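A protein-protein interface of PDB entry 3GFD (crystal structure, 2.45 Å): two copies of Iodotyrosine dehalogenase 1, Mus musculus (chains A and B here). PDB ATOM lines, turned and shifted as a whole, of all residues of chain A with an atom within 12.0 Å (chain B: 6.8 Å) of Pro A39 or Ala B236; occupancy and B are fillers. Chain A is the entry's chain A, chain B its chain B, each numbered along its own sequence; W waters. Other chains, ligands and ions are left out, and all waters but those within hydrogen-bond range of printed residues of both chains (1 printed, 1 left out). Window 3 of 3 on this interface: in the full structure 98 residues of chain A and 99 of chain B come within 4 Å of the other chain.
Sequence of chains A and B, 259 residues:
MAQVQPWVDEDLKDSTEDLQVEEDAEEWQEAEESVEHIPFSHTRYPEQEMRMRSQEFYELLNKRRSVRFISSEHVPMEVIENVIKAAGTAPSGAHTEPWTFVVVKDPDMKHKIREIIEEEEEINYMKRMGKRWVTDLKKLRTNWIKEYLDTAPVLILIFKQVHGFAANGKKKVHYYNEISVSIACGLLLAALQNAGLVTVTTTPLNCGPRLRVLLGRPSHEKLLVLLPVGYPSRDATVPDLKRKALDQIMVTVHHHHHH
Among the printed residues, merely in contact across the chains: His A37 with Thr B237, His A37 with Val B238, Pro A39 with Ala B236, Phe A40 with Val B67, Phe A40 with Pro B232, Phe A40 with Val B238 and His A42 with Pro B232.
Pro A39 touches just one residue of chain B: Ala B236 (3.6 Å).
Of chain A, only Pro A39 (3.6 Å) and Phe A40 (2.8 Å) come within 4 Å of Ala B236.
Val B67 touches one residue of chain A.
No residue of chain A comes within 4 Å of Phe B69.
Of chain A, only Phe A40 (3.9 Å) and His A42 (3.6 Å) come within 4 Å of Pro B232.
No residue of chain A comes within 4 Å of Asp B235.
Thr B237 touches just these residues of chain A: His A37 and Ile A38.
Of chain A, only His A37 (3.5 Å), Ile A38 (2.8 Å) and Phe A40 (3.8 Å) come within 4 Å of Val B238.
Of the printed residues of chain B, Ile A38 touches Thr B237 and Val B238.
Of the printed residues of chain B, His A42 touches Pro B232.
Printed residues of chain B within 4 Å of His A37: Thr B237 and Val B238.
Of the printed residues of chain B, Phe A40 touches Val B67 (3.7 Å), Pro B232 (3.9 Å), Ala B236 (2.8 Å) and Val B238 (3.8 Å).
Ser A41 touches none of the printed residues of chain B.
Glu A36 touches none of the printed residues of chain B.
The nearest printed residue of chain B that does not touch His A37 is Phe B69 (6.0 Å).
Water W1 bridges O of Ser B233 (2.7 Å) and O of Phe A40 (2.9 Å).
Printed residues of chain B that touch a printed residue of chain A: Val B67, Pro B232, Ala B236, Thr B237 and Val B238.
Hydrophobic or aromatic side chains of chain B within 4 Å of the printed part of chain A: Val B67, Pro B232 and Val B238.
Printed residues of chain A that touch a printed residue of chain B: His A37, Ile A38, Pro A39, Phe A40 and His A42.
Hydrophobic or aromatic side chains of chain A that line the printed part of chain B: His A37, Ile A38, Phe A40 and His A42.
Among the printed residues, 10 pairs touch across the chains.
No position is printed for both chains.
Of the 10 pairs that touch across the chains among the printed residues, none has its exchanged pair printed and touching as well.
The backbone carbonyl oxygen of Ile A38 lies close to the side-chain hydroxyl of Thr B237, at 3.5 Å.
The backbone NH (N) of Ile A38 sits at hydrogen-bond distance from the backbone carbonyl oxygen (O) of Val B238, 2.8 Å away.
The backbone carbonyl oxygen (O) of Ala B236 lies within hydrogen-bond range of the backbone NH (N) of Phe A40, 2.8 Å away.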
ATOM      1  N   VAL A  35     -15.527 -11.219 -33.065  1.00  0.00           N
ATOM      2  CA  VAL A  35     -15.024 -12.610 -32.822  1.00  0.00           C
ATOM      3  C   VAL A  35     -15.610 -13.270 -31.543  1.00  0.00           C
ATOM      4  O   VAL A  35     -15.171 -13.016 -30.412  1.00  0.00           O
ATOM      5  CB  VAL A  35     -13.442 -12.832 -32.998  1.00  0.00           C
ATOM      6  CG1 VAL A  35     -13.017 -14.253 -32.592  1.00  0.00           C
ATOM      7  CG2 VAL A  35     -12.965 -12.512 -34.421  1.00  0.00           C
ATOM      8  N   GLU A  36     -16.612 -14.121 -31.750  1.00  0.00           N
ATOM      9  CA  GLU A  36     -17.197 -14.891 -30.651  1.00  0.00           C
ATOM     10  C   GLU A  36     -16.330 -16.118 -30.352  1.00  0.00           C
ATOM     11  O   GLU A  36     -15.457 -16.491 -31.148  1.00  0.00           O
ATOM     12  CB  GLU A  36     -18.653 -15.272 -30.948  1.00  0.00           C
ATOM     13  CG  GLU A  36     -18.789 -16.319 -32.064  1.00  0.00           C
ATOM     14  CD  GLU A  36     -20.027 -17.225 -31.898  1.00  0.00           C
ATOM     15  OE1 GLU A  36     -20.381 -17.967 -32.856  1.00  0.00           O
ATOM     16  OE2 GLU A  36     -20.632 -17.202 -30.801  1.00  0.00           O
ATOM     17  N   HIS A  37     -16.535 -16.716 -29.187  1.00  0.00           N
ATOM     18  CA  HIS A  37     -15.677 -17.811 -28.759  1.00  0.00           C
ATOM     19  C   HIS A  37     -16.531 -19.044 -28.675  1.00  0.00           C
ATOM     20  O   HIS A  37     -17.632 -18.963 -28.215  1.00  0.00           O
ATOM     21  CB  HIS A  37     -15.032 -17.481 -27.420  1.00  0.00           C
ATOM     22  CG  HIS A  37     -13.739 -16.739 -27.550  1.00  0.00           C
ATOM     23  ND1 HIS A  37     -13.641 -15.516 -28.185  1.00  0.00           N
ATOM     24  CD2 HIS A  37     -12.478 -17.062 -27.159  1.00  0.00           C
ATOM     25  CE1 HIS A  37     -12.380 -15.112 -28.167  1.00  0.00           C
ATOM     26  NE2 HIS A  37     -11.656 -16.026 -27.538  1.00  0.00           N
ATOM     27  N   ILE A  38     -16.054 -20.191 -29.123  1.00  0.00           N
ATOM     28  CA  ILE A  38     -16.963 -21.333 -29.251  1.00  0.00           C
ATOM     29  C   ILE A  38     -16.367 -22.494 -28.493  1.00  0.00           C
ATOM     30  O   ILE A  38     -15.174 -22.520 -28.299  1.00  0.00           O
ATOM     31  CB  ILE A  38     -17.175 -21.718 -30.732  1.00  0.00           C
ATOM     32  CG1 ILE A  38     -15.805 -21.913 -31.419  1.00  0.00           C
ATOM     33  CG2 ILE A  38     -17.997 -20.660 -31.405  1.00  0.00           C
ATOM     34  CD1 ILE A  38     -15.863 -22.446 -32.825  1.00  0.00           C
ATOM     35  N   PRO A  39     -17.203 -23.468 -28.084  1.00  0.00           N
ATOM     36  CA  PRO A  39     -16.673 -24.634 -27.367  1.00  0.00           C
ATOM     37  C   PRO A  39     -15.634 -25.394 -28.208  1.00  0.00           C
ATOM     38  O   PRO A  39     -15.718 -25.411 -29.429  1.00  0.00           O
ATOM     39  CB  PRO A  39     -17.914 -25.498 -27.132  1.00  0.00           C
ATOM     40  CG  PRO A  39     -19.082 -24.497 -27.229  1.00  0.00           C
ATOM     41  CD  PRO A  39     -18.666 -23.546 -28.286  1.00  0.00           C
ATOM     42  N   PHE A  40     -14.630 -25.992 -27.566  1.00  0.00           N
ATOM     43  CA  PHE A  40     -13.668 -26.745 -28.325  1.00  0.00           C
ATOM     44  C   PHE A  40     -13.857 -28.205 -28.111  1.00  0.00           C
ATOM     45  O   PHE A  40     -13.985 -28.672 -26.991  1.00  0.00           O
ATOM     46  CB  PHE A  40     -12.236 -26.410 -27.927  1.00  0.00           C
ATOM     47  CG  PHE A  40     -11.215 -27.309 -28.564  1.00  0.00           C
ATOM     48  CD1 PHE A  40     -10.808 -27.099 -29.875  1.00  0.00           C
ATOM     49  CD2 PHE A  40     -10.676 -28.386 -27.856  1.00  0.00           C
ATOM     50  CE1 PHE A  40      -9.837 -27.930 -30.458  1.00  0.00           C
ATOM     51  CE2 PHE A  40      -9.728 -29.235 -28.449  1.00  0.00           C
ATOM     52  CZ  PHE A  40      -9.314 -28.993 -29.754  1.00  0.00           C
ATOM     53  N   SER A  41     -13.781 -28.958 -29.183  1.00  0.00           N
ATOM     54  CA  SER A  41     -13.697 -30.389 -28.985  1.00  0.00           C
ATOM     55  C   SER A  41     -12.675 -31.079 -29.839  1.00  0.00           C
ATOM     56  O   SER A  41     -12.144 -30.526 -30.816  1.00  0.00           O
ATOM     57  CB  SER A  41     -15.064 -31.062 -29.110  1.00  0.00           C
ATOM     58  OG  SER A  41     -15.540 -31.197 -27.798  1.00  0.00           O
ATOM     59  N   HIS A  42     -12.526 -32.348 -29.507  1.00  0.00           N
ATOM     60  CA  HIS A  42     -11.258 -33.001 -29.501  1.00  0.00           C
ATOM     61  C   HIS A  42     -11.509 -34.462 -29.726  1.00  0.00           C
ATOM     62  O   HIS A  42     -12.447 -34.989 -29.182  1.00  0.00           O
ATOM     63  CB  HIS A  42     -10.807 -32.790 -28.079  1.00  0.00           C
ATOM     64  CG  HIS A  42      -9.632 -33.591 -27.677  1.00  0.00           C
ATOM     65  ND1 HIS A  42      -8.411 -33.458 -28.298  1.00  0.00           N
ATOM     66  CD2 HIS A  42      -9.465 -34.484 -26.671  1.00  0.00           C
ATOM     67  CE1 HIS A  42      -7.540 -34.257 -27.703  1.00  0.00           C
ATOM     68  NE2 HIS A  42      -8.156 -34.892 -26.717  1.00  0.00           N
ATOM     69  N   THR A  43     -10.677 -35.134 -30.496  1.00  0.00           N
ATOM     70  CA  THR A  43     -10.749 -36.584 -30.520  1.00  0.00           C
ATOM     71  C   THR A  43      -9.717 -37.076 -29.506  1.00  0.00           C
ATOM     72  O   THR A  43      -8.520 -36.712 -29.589  1.00  0.00           O
ATOM     73  CB  THR A  43     -10.440 -37.132 -31.919  1.00  0.00           C
ATOM     74  OG1 THR A  43     -11.409 -36.619 -32.820  1.00  0.00           O
ATOM     75  CG2 THR A  43     -10.498 -38.664 -31.965  1.00  0.00           C
ATOM     76  N   ARG A  44     -10.173 -37.883 -28.554  1.00  0.00           N
ATOM     77  CA  ARG A  44      -9.264 -38.459 -27.589  1.00  0.00           C
ATOM     78  C   ARG A  44      -9.028 -39.962 -27.907  1.00  0.00           C
ATOM     79  O   ARG A  44      -9.951 -40.665 -28.250  1.00  0.00           O
ATOM     80  CB  ARG A  44      -9.860 -38.300 -26.197  1.00  0.00           C
ATOM     81  CG  ARG A  44      -9.026 -38.849 -25.112  1.00  0.00           C
ATOM     82  CD  ARG A  44      -9.583 -38.461 -23.806  1.00  0.00           C
ATOM     83  NE  ARG A  44      -8.796 -39.077 -22.748  1.00  0.00           N
ATOM     84  CZ  ARG A  44      -8.676 -38.597 -21.517  1.00  0.00           C
ATOM     85  NH1 ARG A  44      -9.283 -37.457 -21.193  1.00  0.00           N
ATOM     86  NH2 ARG A  44      -7.943 -39.267 -20.615  1.00  0.00           N
ATOM     87  N   VAL B  67      -5.254 -24.213 -27.866  1.00  0.00           N
ATOM     88  CA  VAL B  67      -6.215 -24.394 -26.775  1.00  0.00           C
ATOM     89  C   VAL B  67      -5.576 -23.807 -25.514  1.00  0.00           C
ATOM     90  O   VAL B  67      -4.475 -24.252 -25.080  1.00  0.00           O
ATOM     91  CB  VAL B  67      -6.630 -25.904 -26.572  1.00  0.00           C
ATOM     92  CG1 VAL B  67      -7.513 -26.066 -25.340  1.00  0.00           C
ATOM     93  CG2 VAL B  67      -7.344 -26.488 -27.824  1.00  0.00           C
ATOM     94  N   ARG B  68      -6.260 -22.828 -24.915  1.00  0.00           N
ATOM     95  CA  ARG B  68      -5.668 -22.118 -23.781  1.00  0.00           C
ATOM     96  C   ARG B  68      -6.198 -22.598 -22.420  1.00  0.00           C
ATOM     97  O   ARG B  68      -5.927 -21.992 -21.374  1.00  0.00           O
ATOM     98  CB  ARG B  68      -5.778 -20.590 -23.971  1.00  0.00           C
ATOM     99  CG  ARG B  68      -5.084 -20.117 -25.229  1.00  0.00           C
ATOM    100  CD  ARG B  68      -5.143 -18.584 -25.462  1.00  0.00           C
ATOM    101  NE  ARG B  68      -4.324 -18.227 -26.621  1.00  0.00           N
ATOM    102  CZ  ARG B  68      -4.791 -18.171 -27.881  1.00  0.00           C
ATOM    103  NH1 ARG B  68      -6.100 -18.371 -28.129  1.00  0.00           N
ATOM    104  NH2 ARG B  68      -3.957 -17.842 -28.889  1.00  0.00           N
ATOM    105  N   PHE B  69      -6.920 -23.711 -22.441  1.00  0.00           N
ATOM    106  CA  PHE B  69      -7.561 -24.245 -21.254  1.00  0.00           C
ATOM    107  C   PHE B  69      -7.259 -25.731 -21.150  1.00  0.00           C
ATOM    108  O   PHE B  69      -7.793 -26.561 -21.913  1.00  0.00           O
ATOM    109  CB  PHE B  69      -9.063 -23.963 -21.307  1.00  0.00           C
ATOM    110  CG  PHE B  69      -9.355 -22.538 -21.594  1.00  0.00           C
ATOM    111  CD1 PHE B  69      -9.320 -21.590 -20.556  1.00  0.00           C
ATOM    112  CD2 PHE B  69      -9.558 -22.106 -22.924  1.00  0.00           C
ATOM    113  CE1 PHE B  69      -9.557 -20.240 -20.818  1.00  0.00           C
ATOM    114  CE2 PHE B  69      -9.772 -20.757 -23.210  1.00  0.00           C
ATOM    115  CZ  PHE B  69      -9.779 -19.815 -22.150  1.00  0.00           C
ATOM    116  N   ILE B  70      -6.393 -26.066 -20.203  1.00  0.00           N
ATOM    117  CA  ILE B  70      -5.827 -27.386 -20.215  1.00  0.00           C
ATOM    118  C   ILE B  70      -6.106 -28.130 -18.921  1.00  0.00           C
ATOM    119  O   ILE B  70      -5.849 -27.641 -17.811  1.00  0.00           O
ATOM    120  CB  ILE B  70      -4.339 -27.345 -20.656  1.00  0.00           C
ATOM    121  CG1 ILE B  70      -4.329 -27.070 -22.163  1.00  0.00           C
ATOM    122  CG2 ILE B  70      -3.665 -28.708 -20.475  1.00  0.00           C
ATOM    123  CD1 ILE B  70      -3.237 -26.324 -22.595  1.00  0.00           C
ATOM    124  N   PRO B 232      -7.711 -31.120 -23.452  1.00  0.00           N
ATOM    125  CA  PRO B 232      -8.364 -29.827 -23.239  1.00  0.00           C
ATOM    126  C   PRO B 232      -9.250 -29.905 -21.980  1.00  0.00           C
ATOM    127  O   PRO B 232      -9.763 -30.963 -21.671  1.00  0.00           O
ATOM    128  CB  PRO B 232      -9.267 -29.679 -24.481  1.00  0.00           C
ATOM    129  CG  PRO B 232      -9.516 -31.107 -24.918  1.00  0.00           C
ATOM    130  CD  PRO B 232      -8.263 -31.864 -24.598  1.00  0.00           C
ATOM    131  N   SER B 233      -9.457 -28.810 -21.284  1.00  0.00           N
ATOM    132  CA  SER B 233     -10.493 -28.777 -20.273  1.00  0.00           C
ATOM    133  C   SER B 233     -11.847 -29.160 -20.863  1.00  0.00           C
ATOM    134  O   SER B 233     -12.131 -28.857 -22.048  1.00  0.00           O
ATOM    135  CB  SER B 233     -10.595 -27.364 -19.740  1.00  0.00           C
ATOM    136  OG  SER B 233      -9.570 -27.220 -18.795  1.00  0.00           O
ATOM    137  N   ARG B 234     -12.694 -29.786 -20.036  1.00  0.00           N
ATOM    138  CA  ARG B 234     -14.099 -30.038 -20.452  1.00  0.00           C
ATOM    139  C   ARG B 234     -14.819 -28.807 -21.013  1.00  0.00           C
ATOM    140  O   ARG B 234     -15.531 -28.895 -22.009  1.00  0.00           O
ATOM    141  CB  ARG B 234     -14.955 -30.677 -19.357  1.00  0.00           C
ATOM    142  CG  ARG B 234     -16.410 -31.017 -19.893  1.00  0.00           C
ATOM    143  CD  ARG B 234     -17.269 -31.763 -18.855  1.00  0.00           C
ATOM    144  NE  ARG B 234     -16.575 -32.995 -18.466  1.00  0.00           N
ATOM    145  CZ  ARG B 234     -16.753 -33.661 -17.320  1.00  0.00           C
ATOM    146  NH1 ARG B 234     -17.633 -33.235 -16.397  1.00  0.00           N
ATOM    147  NH2 ARG B 234     -16.050 -34.773 -17.107  1.00  0.00           N
ATOM    148  N   ASP B 235     -14.627 -27.653 -20.413  1.00  0.00           N
ATOM    149  CA  ASP B 235     -15.284 -26.456 -20.963  1.00  0.00           C
ATOM    150  C   ASP B 235     -14.347 -25.567 -21.783  1.00  0.00           C
ATOM    151  O   ASP B 235     -14.571 -24.344 -21.860  1.00  0.00           O
ATOM    152  CB  ASP B 235     -15.860 -25.631 -19.829  1.00  0.00           C
ATOM    153  CG  ASP B 235     -14.824 -25.329 -18.775  1.00  0.00           C
ATOM    154  OD1 ASP B 235     -15.029 -24.398 -17.962  1.00  0.00           O
ATOM    155  OD2 ASP B 235     -13.794 -26.030 -18.748  1.00  0.00           O
ATOM    156  N   ALA B 236     -13.300 -26.170 -22.377  1.00  0.00           N
ATOM    157  CA  ALA B 236     -12.375 -25.426 -23.198  1.00  0.00           C
ATOM    158  C   ALA B 236     -13.099 -24.680 -24.293  1.00  0.00           C
ATOM    159  O   ALA B 236     -14.052 -25.177 -24.934  1.00  0.00           O
ATOM    160  CB  ALA B 236     -11.339 -26.336 -23.793  1.00  0.00           C
ATOM    161  N   THR B 237     -12.585 -23.504 -24.568  1.00  0.00           N
ATOM    162  CA  THR B 237     -13.138 -22.646 -25.570  1.00  0.00           C
ATOM    163  C   THR B 237     -12.013 -22.274 -26.582  1.00  0.00           C
ATOM    164  O   THR B 237     -10.821 -22.317 -26.235  1.00  0.00           O
ATOM    165  CB  THR B 237     -13.743 -21.462 -24.755  1.00  0.00           C
ATOM    166  OG1 THR B 237     -15.138 -21.388 -25.016  1.00  0.00           O
ATOM    167  CG2 THR B 237     -13.089 -20.151 -24.945  1.00  0.00           C
ATOM    168  N   VAL B 238     -12.356 -21.937 -27.819  1.00  0.00           N
ATOM    169  CA  VAL B 238     -11.375 -21.339 -28.748  1.00  0.00           C
ATOM    170  C   VAL B 238     -12.069 -20.172 -29.461  1.00  0.00           C
ATOM    171  O   VAL B 238     -13.291 -20.168 -29.580  1.00  0.00           O
ATOM    172  CB  VAL B 238     -10.869 -22.378 -29.821  1.00  0.00           C
ATOM    173  CG1 VAL B 238      -9.952 -23.452 -29.199  1.00  0.00           C
ATOM    174  CG2 VAL B 238     -12.057 -23.075 -30.535  1.00  0.00           C
HETATM  175  O   HOH W   1     -12.760 -29.676 -24.506  1.00  0.00           O
